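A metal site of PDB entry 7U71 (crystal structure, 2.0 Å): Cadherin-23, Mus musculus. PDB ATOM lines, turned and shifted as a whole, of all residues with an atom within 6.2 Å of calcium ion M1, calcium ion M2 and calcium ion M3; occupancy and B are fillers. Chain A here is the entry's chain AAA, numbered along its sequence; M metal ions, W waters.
OD2 of Asp 213 is in hydrogen-bond range of N of Ile 251 (3.2 Å).
The side-chain amide nitrogen (ND2) of Asn 217 lies close to the side-chain carboxylate (OE2) of Glu 182 (3.3 Å).
ND2 of Asn 217 lies close to OD1 of Asp 216 (3.1 Å).
NH1 of Arg 249 sits at hydrogen-bond distance from OD1 of Asn 217 (3.1 Å).
The side-chain carboxylate of Glu 124 lies close to the backbone NH of Arg 181 (2.9 Å).
The backbone carbonyl oxygen (O) of Leu 212 sits at hydrogen-bond distance from the backbone NH (N) of Glu 124 (3.0 Å).
The side-chain hydroxyl (OG) of Ser 255 lies close to the backbone carbonyl oxygen (O) of Asp 250.
The backbone NH (N) of Leu 308 is in hydrogen-bond range of the side-chain carboxylate (OD1) of Asp 302, at 2.9 Å.
Along chain A the residues within 4 Å of calcium ion M1 span positions 124 to 216.
Along chain A the residues within 4 Å of calcium ion M2 span positions 124 to 250.
The nearest printed residue that does not touch calcium ion M2 is Arg 181 (4.4 Å).
The nearest printed residue that does not touch calcium ion M3 is Ser 255 (4.5 Å).
Calcium ion M1 is bound by the side-chain carboxylate (OD1) of Asp 180 (2.3 Å), the side-chain carboxylate (OE1) of Glu 124 (2.3 Å), the side-chain carboxylate (OE2) of Glu 182 (2.3 Å), the side-chain carboxylate (OD2) of Asp 216 (2.4 Å), water W1 (2.4 Å) and water W2 (2.5 Å).
Calcium ion M1 has six donor atoms within binding distance.
Slightly farther from calcium ion M1 lies the side-chain carboxylate (OD1) of Asp 216 (3.1 Å).
Calcium ion M2 is bound by OD1 of Asp 213 (2.3 Å), OE2 of Glu 124 (2.3 Å), OD1 of Asp 250 (2.4 Å), O of Val 214 (2.4 Å), OD1 of Asp 216 (2.4 Å), OE1 of Glu 182 (2.5 Å) and OE2 of Glu 182 (2.7 Å).
Calcium ion M3 is bound by the backbone carbonyl oxygen (O) of Asn 217 (2.3 Å), the side-chain carboxylate (OD2) of Asp 302 (2.4 Å), the side-chain amide oxygen (OD1) of Asn 215 (2.4 Å), the backbone carbonyl oxygen (O) of Asn 254 (2.4 Å), the side-chain carboxylate (OD2) of Asp 248 (2.4 Å), the side-chain carboxylate (OD2) of Asp 250 (2.4 Å) and the side-chain carboxylate (OD1) of Asp 248 (2.6 Å).
Calcium ion M3 has seven donor atoms within binding distance.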
ATOM      1  N   GLU A 124     -24.990  29.600  -1.372  1.00  0.00           N
ATOM      2  CA  GLU A 124     -25.324  28.946  -0.090  1.00  0.00           C
ATOM      3  C   GLU A 124     -24.084  28.959   0.808  1.00  0.00           C
ATOM      4  O   GLU A 124     -24.252  28.753   2.004  1.00  0.00           O
ATOM      5  CB  GLU A 124     -25.868  27.525  -0.330  1.00  0.00           C
ATOM      6  CG  GLU A 124     -24.972  26.600  -1.127  1.00  0.00           C
ATOM      7  CD  GLU A 124     -25.354  25.128  -1.037  1.00  0.00           C
ATOM      8  OE1 GLU A 124     -25.868  24.682   0.051  1.00  0.00           O
ATOM      9  OE2 GLU A 124     -25.115  24.413  -2.038  1.00  0.00           O
ATOM     10  N   LEU A 179     -26.343  29.190   5.466  1.00  0.00           N
ATOM     11  CA  LEU A 179     -27.368  28.804   4.484  1.00  0.00           C
ATOM     12  C   LEU A 179     -27.088  27.392   4.004  1.00  0.00           C
ATOM     13  O   LEU A 179     -25.961  26.921   4.119  1.00  0.00           O
ATOM     14  CB  LEU A 179     -27.409  29.807   3.329  1.00  0.00           C
ATOM     15  CG  LEU A 179     -27.472  31.279   3.740  1.00  0.00           C
ATOM     16  CD1 LEU A 179     -27.236  32.181   2.551  1.00  0.00           C
ATOM     17  CD2 LEU A 179     -28.779  31.609   4.430  1.00  0.00           C
ATOM     18  N   ASP A 180     -28.102  26.770   3.398  1.00  0.00           N
ATOM     19  CA  ASP A 180     -27.963  25.427   2.804  1.00  0.00           C
ATOM     20  C   ASP A 180     -29.041  25.302   1.737  1.00  0.00           C
ATOM     21  O   ASP A 180     -30.203  25.033   2.133  1.00  0.00           O
ATOM     22  CB  ASP A 180     -28.111  24.347   3.888  1.00  0.00           C
ATOM     23  CG  ASP A 180     -27.986  22.955   3.297  1.00  0.00           C
ATOM     24  OD1 ASP A 180     -27.536  22.808   2.120  1.00  0.00           O
ATOM     25  OD2 ASP A 180     -28.290  22.016   4.024  1.00  0.00           O
ATOM     26  N   ARG A 181     -28.670  25.388   0.452  1.00  0.00           N
ATOM     27  CA  ARG A 181     -29.617  25.262  -0.691  1.00  0.00           C
ATOM     28  C   ARG A 181     -30.350  23.911  -0.629  1.00  0.00           C
ATOM     29  O   ARG A 181     -31.544  23.865  -1.026  1.00  0.00           O
ATOM     30  CB  ARG A 181     -28.902  25.373  -2.032  1.00  0.00           C
ATOM     31  CG  ARG A 181     -29.828  25.478  -3.243  1.00  0.00           C
ATOM     32  CD  ARG A 181     -29.290  24.871  -4.517  1.00  0.00           C
ATOM     33  NE  ARG A 181     -29.118  23.446  -4.340  1.00  0.00           N
ATOM     34  CZ  ARG A 181     -30.087  22.526  -4.356  1.00  0.00           C
ATOM     35  NH1 ARG A 181     -31.334  22.855  -4.638  1.00  0.00           N
ATOM     36  NH2 ARG A 181     -29.774  21.274  -4.088  1.00  0.00           N
ATOM     37  N   GLU A 182     -29.686  22.864  -0.146  1.00  0.00           N
ATOM     38  CA  GLU A 182     -30.291  21.488  -0.071  1.00  0.00           C
ATOM     39  C   GLU A 182     -31.396  21.440   0.999  1.00  0.00           C
ATOM     40  O   GLU A 182     -32.189  20.492   0.959  1.00  0.00           O
ATOM     41  CB  GLU A 182     -29.228  20.425   0.224  1.00  0.00           C
ATOM     42  CG  GLU A 182     -28.446  20.031  -1.006  1.00  0.00           C
ATOM     43  CD  GLU A 182     -27.434  21.026  -1.541  1.00  0.00           C
ATOM     44  OE1 GLU A 182     -27.442  21.262  -2.759  1.00  0.00           O
ATOM     45  OE2 GLU A 182     -26.671  21.607  -0.714  1.00  0.00           O
ATOM     46  N   GLU A 183     -31.443  22.388   1.937  1.00  0.00           N
ATOM     47  CA  GLU A 183     -32.518  22.489   2.950  1.00  0.00           C
ATOM     48  C   GLU A 183     -33.562  23.488   2.438  1.00  0.00           C
ATOM     49  O   GLU A 183     -34.744  23.126   2.410  1.00  0.00           O
ATOM     50  CB  GLU A 183     -31.967  22.771   4.348  1.00  0.00           C
ATOM     51  CG  GLU A 183     -33.063  23.055   5.377  1.00  0.00           C
ATOM     52  CD  GLU A 183     -34.117  21.974   5.623  1.00  0.00           C
ATOM     53  OE1 GLU A 183     -33.767  20.782   5.509  1.00  0.00           O
ATOM     54  OE2 GLU A 183     -35.314  22.337   5.924  1.00  0.00           O
ATOM     55  N   LEU A 212     -28.173  30.129  -4.393  1.00  0.00           N
ATOM     56  CA  LEU A 212     -27.423  29.442  -5.477  1.00  0.00           C
ATOM     57  C   LEU A 212     -26.653  28.250  -4.937  1.00  0.00           C
ATOM     58  O   LEU A 212     -26.124  28.292  -3.784  1.00  0.00           O
ATOM     59  CB  LEU A 212     -26.494  30.423  -6.197  1.00  0.00           C
ATOM     60  CG  LEU A 212     -27.223  31.696  -6.626  1.00  0.00           C
ATOM     61  CD1 LEU A 212     -26.240  32.788  -6.970  1.00  0.00           C
ATOM     62  CD2 LEU A 212     -28.184  31.369  -7.759  1.00  0.00           C
ATOM     63  N   ASP A 213     -26.541  27.233  -5.801  1.00  0.00           N
ATOM     64  CA  ASP A 213     -25.897  25.960  -5.407  1.00  0.00           C
ATOM     65  C   ASP A 213     -24.390  26.124  -5.345  1.00  0.00           C
ATOM     66  O   ASP A 213     -23.818  26.767  -6.198  1.00  0.00           O
ATOM     67  CB  ASP A 213     -26.271  24.827  -6.366  1.00  0.00           C
ATOM     68  CG  ASP A 213     -25.913  23.451  -5.851  1.00  0.00           C
ATOM     69  OD1 ASP A 213     -26.178  23.185  -4.657  1.00  0.00           O
ATOM     70  OD2 ASP A 213     -25.344  22.663  -6.674  1.00  0.00           O
ATOM     71  N   VAL A 214     -23.784  25.478  -4.360  1.00  0.00           N
ATOM     72  CA  VAL A 214     -22.330  25.196  -4.300  1.00  0.00           C
ATOM     73  C   VAL A 214     -22.187  23.672  -4.364  1.00  0.00           C
ATOM     74  O   VAL A 214     -23.098  22.950  -3.899  1.00  0.00           O
ATOM     75  CB  VAL A 214     -21.748  25.800  -3.011  1.00  0.00           C
ATOM     76  CG1 VAL A 214     -20.334  25.314  -2.771  1.00  0.00           C
ATOM     77  CG2 VAL A 214     -21.831  27.343  -3.099  1.00  0.00           C
ATOM     78  N   ASN A 215     -21.057  23.196  -4.911  1.00  0.00           N
ATOM     79  CA  ASN A 215     -20.767  21.746  -4.963  1.00  0.00           C
ATOM     80  C   ASN A 215     -20.303  21.313  -3.586  1.00  0.00           C
ATOM     81  O   ASN A 215     -19.086  21.202  -3.359  1.00  0.00           O
ATOM     82  CB  ASN A 215     -19.721  21.377  -6.008  1.00  0.00           C
ATOM     83  CG  ASN A 215     -19.741  19.889  -6.267  1.00  0.00           C
ATOM     84  OD1 ASN A 215     -20.776  19.221  -6.083  1.00  0.00           O
ATOM     85  ND2 ASN A 215     -18.600  19.345  -6.670  1.00  0.00           N
ATOM     86  N   ASP A 216     -21.238  21.011  -2.690  1.00  0.00           N
ATOM     87  CA  ASP A 216     -20.849  20.677  -1.301  1.00  0.00           C
ATOM     88  C   ASP A 216     -21.365  19.289  -0.890  1.00  0.00           C
ATOM     89  O   ASP A 216     -21.271  19.014   0.304  1.00  0.00           O
ATOM     90  CB  ASP A 216     -21.295  21.799  -0.362  1.00  0.00           C
ATOM     91  CG  ASP A 216     -22.789  22.123  -0.330  1.00  0.00           C
ATOM     92  OD1 ASP A 216     -23.540  21.611  -1.147  1.00  0.00           O
ATOM     93  OD2 ASP A 216     -23.174  22.827   0.585  1.00  0.00           O
ATOM     94  N   ASN A 217     -21.882  18.494  -1.837  1.00  0.00           N
ATOM     95  CA  ASN A 217     -22.293  17.082  -1.616  1.00  0.00           C
ATOM     96  C   ASN A 217     -21.560  16.150  -2.579  1.00  0.00           C
ATOM     97  O   ASN A 217     -21.528  16.382  -3.805  1.00  0.00           O
ATOM     98  CB  ASN A 217     -23.794  16.849  -1.743  1.00  0.00           C
ATOM     99  CG  ASN A 217     -24.561  17.589  -0.680  1.00  0.00           C
ATOM    100  OD1 ASN A 217     -24.810  17.064   0.393  1.00  0.00           O
ATOM    101  ND2 ASN A 217     -24.864  18.849  -0.930  1.00  0.00           N
ATOM    102  N   PRO A 218     -20.895  15.111  -2.029  1.00  0.00           N
ATOM    103  CA  PRO A 218     -20.184  14.136  -2.827  1.00  0.00           C
ATOM    104  C   PRO A 218     -21.175  13.160  -3.455  1.00  0.00           C
ATOM    105  O   PRO A 218     -22.290  12.953  -2.977  1.00  0.00           O
ATOM    106  CB  PRO A 218     -19.272  13.455  -1.808  1.00  0.00           C
ATOM    107  CG  PRO A 218     -20.066  13.486  -0.515  1.00  0.00           C
ATOM    108  CD  PRO A 218     -20.831  14.801  -0.599  1.00  0.00           C
ATOM    109  N   PRO A 219     -20.756  12.447  -4.500  1.00  0.00           N
ATOM    110  CA  PRO A 219     -21.493  11.276  -4.946  1.00  0.00           C
ATOM    111  C   PRO A 219     -21.592  10.308  -3.764  1.00  0.00           C
ATOM    112  O   PRO A 219     -20.707  10.242  -2.955  1.00  0.00           O
ATOM    113  CB  PRO A 219     -20.668  10.693  -6.102  1.00  0.00           C
ATOM    114  CG  PRO A 219     -19.693  11.757  -6.479  1.00  0.00           C
ATOM    115  CD  PRO A 219     -19.511  12.650  -5.256  1.00  0.00           C
ATOM    116  N   ASP A 248     -26.357  12.269  -5.949  1.00  0.00           N
ATOM    117  CA  ASP A 248     -25.646  13.494  -5.519  1.00  0.00           C
ATOM    118  C   ASP A 248     -26.710  14.536  -5.210  1.00  0.00           C
ATOM    119  O   ASP A 248     -27.551  14.800  -6.057  1.00  0.00           O
ATOM    120  CB  ASP A 248     -24.633  13.894  -6.567  1.00  0.00           C
ATOM    121  CG  ASP A 248     -23.707  15.026  -6.163  1.00  0.00           C
ATOM    122  OD1 ASP A 248     -24.226  16.019  -5.613  1.00  0.00           O
ATOM    123  OD2 ASP A 248     -22.502  14.937  -6.544  1.00  0.00           O
ATOM    124  N   ARG A 249     -26.643  15.120  -4.025  1.00  0.00           N
ATOM    125  CA  ARG A 249     -27.685  16.031  -3.516  1.00  0.00           C
ATOM    126  C   ARG A 249     -27.619  17.426  -4.150  1.00  0.00           C
ATOM    127  O   ARG A 249     -28.547  18.223  -3.886  1.00  0.00           O
ATOM    128  CB  ARG A 249     -27.537  16.121  -1.991  1.00  0.00           C
ATOM    129  CG  ARG A 249     -28.007  14.858  -1.267  1.00  0.00           C
ATOM    130  CD  ARG A 249     -27.910  14.974   0.241  1.00  0.00           C
ATOM    131  NE  ARG A 249     -28.975  15.753   0.862  1.00  0.00           N
ATOM    132  CZ  ARG A 249     -28.816  16.857   1.600  1.00  0.00           C
ATOM    133  NH1 ARG A 249     -27.621  17.414   1.752  1.00  0.00           N
ATOM    134  NH2 ARG A 249     -29.875  17.405   2.164  1.00  0.00           N
ATOM    135  N   ASP A 250     -26.586  17.753  -4.924  1.00  0.00           N
ATOM    136  CA  ASP A 250     -26.455  19.118  -5.493  1.00  0.00           C
ATOM    137  C   ASP A 250     -27.326  19.158  -6.737  1.00  0.00           C
ATOM    138  O   ASP A 250     -28.098  18.233  -6.919  1.00  0.00           O
ATOM    139  CB  ASP A 250     -24.989  19.490  -5.750  1.00  0.00           C
ATOM    140  CG  ASP A 250     -24.147  19.423  -4.493  1.00  0.00           C
ATOM    141  OD1 ASP A 250     -24.525  20.062  -3.486  1.00  0.00           O
ATOM    142  OD2 ASP A 250     -23.133  18.749  -4.520  1.00  0.00           O
ATOM    143  N   ILE A 251     -27.205  20.192  -7.576  1.00  0.00           N
ATOM    144  CA  ILE A 251     -28.042  20.338  -8.794  1.00  0.00           C
ATOM    145  C   ILE A 251     -27.152  20.726  -9.974  1.00  0.00           C
ATOM    146  O   ILE A 251     -25.981  21.141  -9.711  1.00  0.00           O
ATOM    147  CB  ILE A 251     -29.163  21.358  -8.549  1.00  0.00           C
ATOM    148  CG1 ILE A 251     -28.602  22.731  -8.132  1.00  0.00           C
ATOM    149  CG2 ILE A 251     -30.168  20.789  -7.565  1.00  0.00           C
ATOM    150  CD1 ILE A 251     -29.626  23.852  -8.183  1.00  0.00           C
ATOM    151  N   ILE A 253     -24.575  20.901 -12.894  1.00  0.00           N
ATOM    152  CA  ILE A 253     -23.286  20.183 -13.105  1.00  0.00           C
ATOM    153  C   ILE A 253     -22.725  19.651 -11.785  1.00  0.00           C
ATOM    154  O   ILE A 253     -21.917  18.699 -11.858  1.00  0.00           O
ATOM    155  CB  ILE A 253     -22.173  20.993 -13.831  1.00  0.00           C
ATOM    156  CG1 ILE A 253     -22.085  22.447 -13.384  1.00  0.00           C
ATOM    157  CG2 ILE A 253     -22.299  20.860 -15.348  1.00  0.00           C
ATOM    158  CD1 ILE A 253     -21.702  22.625 -11.968  1.00  0.00           C
ATOM    159  N   ASN A 254     -23.140  20.198 -10.634  1.00  0.00           N
ATOM    160  CA  ASN A 254     -22.628  19.752  -9.316  1.00  0.00           C
ATOM    161  C   ASN A 254     -23.148  18.329  -9.019  1.00  0.00           C
ATOM    162  O   ASN A 254     -22.621  17.704  -8.105  1.00  0.00           O
ATOM    163  CB  ASN A 254     -22.969  20.725  -8.185  1.00  0.00           C
ATOM    164  CG  ASN A 254     -22.334  22.084  -8.422  1.00  0.00           C
ATOM    165  OD1 ASN A 254     -21.213  22.180  -8.935  1.00  0.00           O
ATOM    166  ND2 ASN A 254     -23.014  23.140  -8.000  1.00  0.00           N
ATOM    167  N   SER A 255     -24.132  17.820  -9.764  1.00  0.00           N
ATOM    168  CA  SER A 255     -24.647  16.448  -9.532  1.00  0.00           C
ATOM    169  C   SER A 255     -24.527  15.553 -10.759  1.00  0.00           C
ATOM    170  O   SER A 255     -25.153  14.484 -10.736  1.00  0.00           O
ATOM    171  CB  SER A 255     -26.046  16.514  -9.045  1.00  0.00           C
ATOM    172  OG  SER A 255     -26.884  17.143  -9.972  1.00  0.00           O
ATOM    173  N   LEU A 257     -22.505  12.988 -12.767  1.00  0.00           N
ATOM    174  CA  LEU A 257     -21.508  12.015 -12.263  1.00  0.00           C
ATOM    175  C   LEU A 257     -20.731  11.367 -13.413  1.00  0.00           C
ATOM    176  O   LEU A 257     -21.352  11.060 -14.454  1.00  0.00           O
ATOM    177  CB  LEU A 257     -22.269  10.972 -11.465  1.00  0.00           C
ATOM    178  CG  LEU A 257     -22.959  11.546 -10.220  1.00  0.00           C
ATOM    179  CD1 LEU A 257     -23.472  10.423  -9.317  1.00  0.00           C
ATOM    180  CD2 LEU A 257     -22.021  12.453  -9.461  1.00  0.00           C
ATOM    181  N   ASP A 302     -18.178  13.889  -9.344  1.00  0.00           N
ATOM    182  CA  ASP A 302     -19.153  14.861  -9.892  1.00  0.00           C
ATOM    183  C   ASP A 302     -18.385  15.846 -10.778  1.00  0.00           C
ATOM    184  O   ASP A 302     -17.165  15.812 -10.759  1.00  0.00           O
ATOM    185  CB  ASP A 302     -19.975  15.546  -8.795  1.00  0.00           C
ATOM    186  CG  ASP A 302     -19.212  16.330  -7.737  1.00  0.00           C
ATOM    187  OD1 ASP A 302     -18.073  16.788  -7.991  1.00  0.00           O
ATOM    188  OD2 ASP A 302     -19.799  16.496  -6.635  1.00  0.00           O
ATOM    189  N   GLY A 304     -18.675  19.314 -10.600  1.00  0.00           N
ATOM    190  CA  GLY A 304     -18.621  20.654  -9.957  1.00  0.00           C
ATOM    191  C   GLY A 304     -17.218  21.047  -9.497  1.00  0.00           C
ATOM    192  O   GLY A 304     -16.259  20.319  -9.803  1.00  0.00           O
ATOM    193  N   LEU A 308     -15.814  16.516  -6.202  1.00  0.00           N
ATOM    194  CA  LEU A 308     -16.007  15.600  -5.059  1.00  0.00           C
ATOM    195  C   LEU A 308     -16.158  14.187  -5.615  1.00  0.00           C
ATOM    196  O   LEU A 308     -16.681  14.032  -6.714  1.00  0.00           O
ATOM    197  CB  LEU A 308     -17.262  16.032  -4.285  1.00  0.00           C
ATOM    198  CG  LEU A 308     -17.166  17.429  -3.679  1.00  0.00           C
ATOM    199  CD1 LEU A 308     -18.466  17.786  -2.935  1.00  0.00           C
ATOM    200  CD2 LEU A 308     -15.949  17.514  -2.775  1.00  0.00           C
HETATM  201 CA    CA M   1     -25.534  22.628   1.021  1.00  0.00          CA
HETATM  202 CA    CA M   2     -25.127  22.271  -2.875  1.00  0.00          CA
HETATM  203 CA    CA M   3     -21.946  17.168  -5.890  1.00  0.00          CA
HETATM  204  O   HOH W   1     -25.086  20.423   1.887  1.00  0.00           O
HETATM  205  O   HOH W   2     -24.645  23.633   3.090  1.00  0.00           O
